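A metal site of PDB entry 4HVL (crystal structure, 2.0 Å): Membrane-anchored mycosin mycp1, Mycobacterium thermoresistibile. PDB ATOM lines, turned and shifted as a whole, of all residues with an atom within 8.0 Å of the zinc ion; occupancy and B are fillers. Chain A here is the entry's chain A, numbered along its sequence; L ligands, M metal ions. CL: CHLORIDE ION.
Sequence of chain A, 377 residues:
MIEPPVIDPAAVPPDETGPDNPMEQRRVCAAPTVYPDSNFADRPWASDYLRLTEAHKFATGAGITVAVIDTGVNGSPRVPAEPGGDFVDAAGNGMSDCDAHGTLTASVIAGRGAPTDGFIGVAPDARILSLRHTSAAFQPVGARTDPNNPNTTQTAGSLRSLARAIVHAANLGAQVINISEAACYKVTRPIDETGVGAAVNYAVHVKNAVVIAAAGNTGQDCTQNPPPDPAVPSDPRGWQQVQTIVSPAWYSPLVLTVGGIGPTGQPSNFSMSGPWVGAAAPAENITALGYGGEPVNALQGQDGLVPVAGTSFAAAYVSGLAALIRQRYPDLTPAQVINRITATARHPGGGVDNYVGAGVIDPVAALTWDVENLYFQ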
ATOM      1  N   ILE A  69       0.179  10.417  20.237  1.00  0.00           N
ATOM      2  CA  ILE A  69      -0.459   9.183  20.685  1.00  0.00           C
ATOM      3  C   ILE A  69      -0.320   9.199  22.212  1.00  0.00           C
ATOM      4  O   ILE A  69       0.777   9.096  22.746  1.00  0.00           O
ATOM      5  CB  ILE A  69       0.203   7.939  20.055  1.00  0.00           C
ATOM      6  CG1 ILE A  69       0.245   8.096  18.526  1.00  0.00           C
ATOM      7  CG2 ILE A  69      -0.516   6.671  20.497  1.00  0.00           C
ATOM      8  CD1 ILE A  69       0.702   6.858  17.785  1.00  0.00           C
ATOM      9  N   ASP A  70      -1.450   9.349  22.893  1.00  0.00           N
ATOM     10  CA  ASP A  70      -1.464   9.664  24.317  1.00  0.00           C
ATOM     11  C   ASP A  70      -2.908   9.366  24.831  1.00  0.00           C
ATOM     12  O   ASP A  70      -3.514   8.395  24.377  1.00  0.00           O
ATOM     13  CB  ASP A  70      -1.042  11.131  24.493  1.00  0.00           C
ATOM     14  CG  ASP A  70      -0.522  11.466  25.877  1.00  0.00           C
ATOM     15  OD1 ASP A  70      -1.317  11.276  26.846  1.00  0.00           O
ATOM     16  OD2 ASP A  70       0.648  11.949  25.994  1.00  0.00           O
ATOM     17  N   THR A  71      -3.453  10.176  25.741  1.00  0.00           N
ATOM     18  CA  THR A  71      -4.748   9.881  26.362  1.00  0.00           C
ATOM     19  C   THR A  71      -5.878  10.765  25.769  1.00  0.00           C
ATOM     20  O   THR A  71      -6.914  10.955  26.415  1.00  0.00           O
ATOM     21  CB  THR A  71      -4.700  10.110  27.885  1.00  0.00           C
ATOM     22  OG1 THR A  71      -4.513  11.511  28.140  1.00  0.00           O
ATOM     23  CG2 THR A  71      -3.578   9.309  28.536  1.00  0.00           C
ATOM     24  N   PHE A  87      -8.489   4.754  20.229  1.00  0.00           N
ATOM     25  CA  PHE A  87      -8.170   3.338  20.349  1.00  0.00           C
ATOM     26  C   PHE A  87      -8.518   2.809  21.732  1.00  0.00           C
ATOM     27  O   PHE A  87      -8.134   1.725  22.090  1.00  0.00           O
ATOM     28  CB  PHE A  87      -6.690   3.137  20.005  1.00  0.00           C
ATOM     29  CG  PHE A  87      -6.372   3.525  18.572  1.00  0.00           C
ATOM     30  CD1 PHE A  87      -6.350   4.839  18.187  1.00  0.00           C
ATOM     31  CD2 PHE A  87      -6.146   2.552  17.623  1.00  0.00           C
ATOM     32  CE1 PHE A  87      -6.104   5.194  16.872  1.00  0.00           C
ATOM     33  CE2 PHE A  87      -5.888   2.900  16.304  1.00  0.00           C
ATOM     34  CZ  PHE A  87      -5.857   4.221  15.933  1.00  0.00           C
ATOM     35  N   VAL A  88      -9.292   3.593  22.494  1.00  0.00           N
ATOM     36  CA  VAL A  88      -9.828   3.207  23.812  1.00  0.00           C
ATOM     37  C   VAL A  88     -11.338   3.076  23.734  1.00  0.00           C
ATOM     38  O   VAL A  88     -11.909   1.997  23.992  1.00  0.00           O
ATOM     39  CB  VAL A  88      -9.418   4.275  24.870  1.00  0.00           C
ATOM     40  CG1 VAL A  88     -10.077   4.014  26.221  1.00  0.00           C
ATOM     41  CG2 VAL A  88      -7.907   4.289  24.984  1.00  0.00           C
ATOM     42  N   LEU A 131      -4.504  11.247  18.951  1.00  0.00           N
ATOM     43  CA  LEU A 131      -4.927   9.843  18.939  1.00  0.00           C
ATOM     44  C   LEU A 131      -4.937   9.373  20.377  1.00  0.00           C
ATOM     45  O   LEU A 131      -3.901   9.446  21.072  1.00  0.00           O
ATOM     46  CB  LEU A 131      -3.943   8.986  18.160  1.00  0.00           C
ATOM     47  CG  LEU A 131      -3.795   9.220  16.661  1.00  0.00           C
ATOM     48  CD1 LEU A 131      -2.843  10.385  16.362  1.00  0.00           C
ATOM     49  CD2 LEU A 131      -3.291   7.952  15.990  1.00  0.00           C
ATOM     50  N   ARG A 132      -6.093   8.914  20.848  1.00  0.00           N
ATOM     51  CA  ARG A 132      -6.173   8.361  22.184  1.00  0.00           C
ATOM     52  C   ARG A 132      -5.876   6.852  22.103  1.00  0.00           C
ATOM     53  O   ARG A 132      -6.624   6.094  21.480  1.00  0.00           O
ATOM     54  CB  ARG A 132      -7.517   8.632  22.871  1.00  0.00           C
ATOM     55  CG  ARG A 132      -7.622   7.898  24.199  1.00  0.00           C
ATOM     56  CD  ARG A 132      -8.642   8.457  25.144  1.00  0.00           C
ATOM     57  NE  ARG A 132     -10.005   8.203  24.666  1.00  0.00           N
ATOM     58  CZ  ARG A 132     -11.094   8.442  25.391  1.00  0.00           C
ATOM     59  NH1 ARG A 132     -10.999   8.923  26.608  1.00  0.00           N
ATOM     60  NH2 ARG A 132     -12.288   8.209  24.860  1.00  0.00           N
ATOM     61  N   HIS A 133      -4.798   6.455  22.754  1.00  0.00           N
ATOM     62  CA  HIS A 133      -4.429   5.057  22.870  1.00  0.00           C
ATOM     63  C   HIS A 133      -4.566   4.498  24.305  1.00  0.00           C
ATOM     64  O   HIS A 133      -4.757   3.288  24.453  1.00  0.00           O
ATOM     65  CB  HIS A 133      -3.006   4.827  22.341  1.00  0.00           C
ATOM     66  CG  HIS A 133      -2.533   3.435  22.534  1.00  0.00           C
ATOM     67  ND1 HIS A 133      -1.749   3.061  23.607  1.00  0.00           N
ATOM     68  CD2 HIS A 133      -2.826   2.284  21.874  1.00  0.00           C
ATOM     69  CE1 HIS A 133      -1.543   1.762  23.567  1.00  0.00           C
ATOM     70  NE2 HIS A 133      -2.187   1.274  22.526  1.00  0.00           N
ATOM     71  N   THR A 134      -4.475   5.356  25.323  1.00  0.00           N
ATOM     72  CA  THR A 134      -4.547   4.923  26.728  1.00  0.00           C
ATOM     73  C   THR A 134      -5.499   5.772  27.533  1.00  0.00           C
ATOM     74  O   THR A 134      -5.627   6.959  27.264  1.00  0.00           O
ATOM     75  CB  THR A 134      -3.152   5.012  27.418  1.00  0.00           C
ATOM     76  OG1 THR A 134      -2.350   3.935  26.947  1.00  0.00           O
ATOM     77  CG2 THR A 134      -3.218   4.858  28.924  1.00  0.00           C
ATOM     78  N   SER A 135      -6.162   5.150  28.523  1.00  0.00           N
ATOM     79  CA  SER A 135      -6.841   5.878  29.614  1.00  0.00           C
ATOM     80  C   SER A 135      -6.994   5.036  30.866  1.00  0.00           C
ATOM     81  O   SER A 135      -7.573   3.940  30.814  1.00  0.00           O
ATOM     82  CB  SER A 135      -8.237   6.373  29.227  1.00  0.00           C
ATOM     83  OG  SER A 135      -8.899   6.928  30.382  1.00  0.00           O
ATOM     84  N   SER A 158      -2.821  -3.938  24.265  1.00  0.00           N
ATOM     85  CA  SER A 158      -2.444  -2.537  24.148  1.00  0.00           C
ATOM     86  C   SER A 158      -1.362  -2.342  23.035  1.00  0.00           C
ATOM     87  O   SER A 158      -1.404  -1.377  22.272  1.00  0.00           O
ATOM     88  CB  SER A 158      -1.992  -2.012  25.508  1.00  0.00           C
ATOM     89  OG  SER A 158      -1.331  -0.773  25.423  1.00  0.00           O
ATOM     90  N   LEU A 159      -0.447  -3.279  22.906  1.00  0.00           N
ATOM     91  CA  LEU A 159       0.560  -3.227  21.822  1.00  0.00           C
ATOM     92  C   LEU A 159      -0.063  -3.517  20.441  1.00  0.00           C
ATOM     93  O   LEU A 159       0.343  -2.922  19.446  1.00  0.00           O
ATOM     94  CB  LEU A 159       1.719  -4.172  22.109  1.00  0.00           C
ATOM     95  CG  LEU A 159       2.687  -3.685  23.189  1.00  0.00           C
ATOM     96  CD1 LEU A 159       3.626  -4.798  23.625  1.00  0.00           C
ATOM     97  CD2 LEU A 159       3.505  -2.495  22.739  1.00  0.00           C
ATOM     98  N   SER A 161      -3.210  -2.610  19.643  1.00  0.00           N
ATOM     99  CA  SER A 161      -3.904  -1.329  19.290  1.00  0.00           C
ATOM    100  C   SER A 161      -2.913  -0.185  18.967  1.00  0.00           C
ATOM    101  O   SER A 161      -3.181   0.682  18.115  1.00  0.00           O
ATOM    102  CB  SER A 161      -4.883  -0.914  20.380  1.00  0.00           C
ATOM    103  OG  SER A 161      -4.219  -0.477  21.540  1.00  0.00           O
ATOM    104  N   LEU A 162      -1.766  -0.196  19.626  1.00  0.00           N
ATOM    105  CA  LEU A 162      -0.720   0.743  19.334  1.00  0.00           C
ATOM    106  C   LEU A 162      -0.180   0.602  17.912  1.00  0.00           C
ATOM    107  O   LEU A 162       0.056   1.591  17.230  1.00  0.00           O
ATOM    108  CB  LEU A 162       0.450   0.556  20.303  1.00  0.00           C
ATOM    109  CG  LEU A 162       1.570   1.544  20.045  1.00  0.00           C
ATOM    110  CD1 LEU A 162       1.091   2.963  20.342  1.00  0.00           C
ATOM    111  CD2 LEU A 162       2.802   1.191  20.863  1.00  0.00           C
ATOM    112  N   ILE A 179       4.991   9.371  20.537  1.00  0.00           N
ATOM    113  CA  ILE A 179       4.378   8.218  21.190  1.00  0.00           C
ATOM    114  C   ILE A 179       4.697   8.272  22.687  1.00  0.00           C
ATOM    115  O   ILE A 179       5.834   8.083  23.101  1.00  0.00           O
ATOM    116  CB  ILE A 179       4.906   6.888  20.597  1.00  0.00           C
ATOM    117  CG1 ILE A 179       4.714   6.878  19.079  1.00  0.00           C
ATOM    118  CG2 ILE A 179       4.184   5.704  21.253  1.00  0.00           C
ATOM    119  CD1 ILE A 179       5.021   5.562  18.366  1.00  0.00           C
ATOM    120  N   SER A 180       3.674   8.552  23.476  1.00  0.00           N
ATOM    121  CA  SER A 180       3.800   8.614  24.911  1.00  0.00           C
ATOM    122  C   SER A 180       3.726   7.216  25.512  1.00  0.00           C
ATOM    123  O   SER A 180       4.161   7.003  26.625  1.00  0.00           O
ATOM    124  CB  SER A 180       2.716   9.511  25.540  1.00  0.00           C
ATOM    125  OG  SER A 180       2.717  10.823  24.981  1.00  0.00           O
ATOM    126  N   GLU A 181       3.175   6.249  24.772  1.00  0.00           N
ATOM    127  CA  GLU A 181       3.008   4.873  25.284  1.00  0.00           C
ATOM    128  C   GLU A 181       4.383   4.257  25.531  1.00  0.00           C
ATOM    129  O   GLU A 181       5.269   4.356  24.673  1.00  0.00           O
ATOM    130  CB  GLU A 181       2.215   4.008  24.276  1.00  0.00           C
ATOM    131  CG  GLU A 181       2.103   2.529  24.600  1.00  0.00           C
ATOM    132  CD  GLU A 181       1.380   2.249  25.905  1.00  0.00           C
ATOM    133  OE1 GLU A 181       0.410   2.945  26.225  1.00  0.00           O
ATOM    134  OE2 GLU A 181       1.801   1.313  26.614  1.00  0.00           O
ATOM    135  N   ALA A 182       4.567   3.643  26.694  1.00  0.00           N
ATOM    136  CA  ALA A 182       5.777   2.890  26.953  1.00  0.00           C
ATOM    137  C   ALA A 182       5.357   1.636  27.686  1.00  0.00           C
ATOM    138  O   ALA A 182       5.256   1.617  28.907  1.00  0.00           O
ATOM    139  CB  ALA A 182       6.769   3.696  27.770  1.00  0.00           C
ATOM    140  N   ALA A 183       5.112   0.566  26.909  1.00  0.00           N
ATOM    141  CA  ALA A 183       4.599  -0.697  27.472  1.00  0.00           C
ATOM    142  C   ALA A 183       5.745  -1.582  27.895  1.00  0.00           C
ATOM    143  O   ALA A 183       6.694  -1.765  27.155  1.00  0.00           O
ATOM    144  CB  ALA A 183       3.778  -1.418  26.434  1.00  0.00           C
HETATM  145 CL    CL L   1      -0.476   6.432  24.985  1.00  0.00          CL
HETATM  146 ZN    ZN M   1      -0.982   4.082  25.325  1.00  0.00          ZN
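The zinc ion is bound by OE1 of Glu 181 (2.0 Å), OG1 of Thr 134 (2.1 Å), ND1 of His 133 (2.1 Å) and CL of the ligand (2.4 Å).
The zinc ion has four donor atoms within binding distance.
Within 4 Å of the zinc ion: His 133, Thr 134 and Glu 181.
The nearest printed residue that does not touch the zinc ion is Ser 158 (4.9 Å).
The backbone carbonyl oxygen (O) of Ser 158 is in hydrogen-bond range of a ring nitrogen (NE2) of His 133, at 2.8 Å.
NE2 of His 133 sits at hydrogen-bond distance from OG of Ser 161 (2.9 Å).
N of His 133 sits at hydrogen-bond distance from O of Asp 70, 2.8 Å away.
OE2 of Glu 181 lies close to N of Ala 183 (3.4 Å).
A ring nitrogen (NE2) of His 133 lies within hydrogen-bond range of the backbone NH (N) of Leu 162 (3.3 Å).
N of Thr 134 lies within hydrogen-bond range of O of Asp 70 (3.3 Å).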
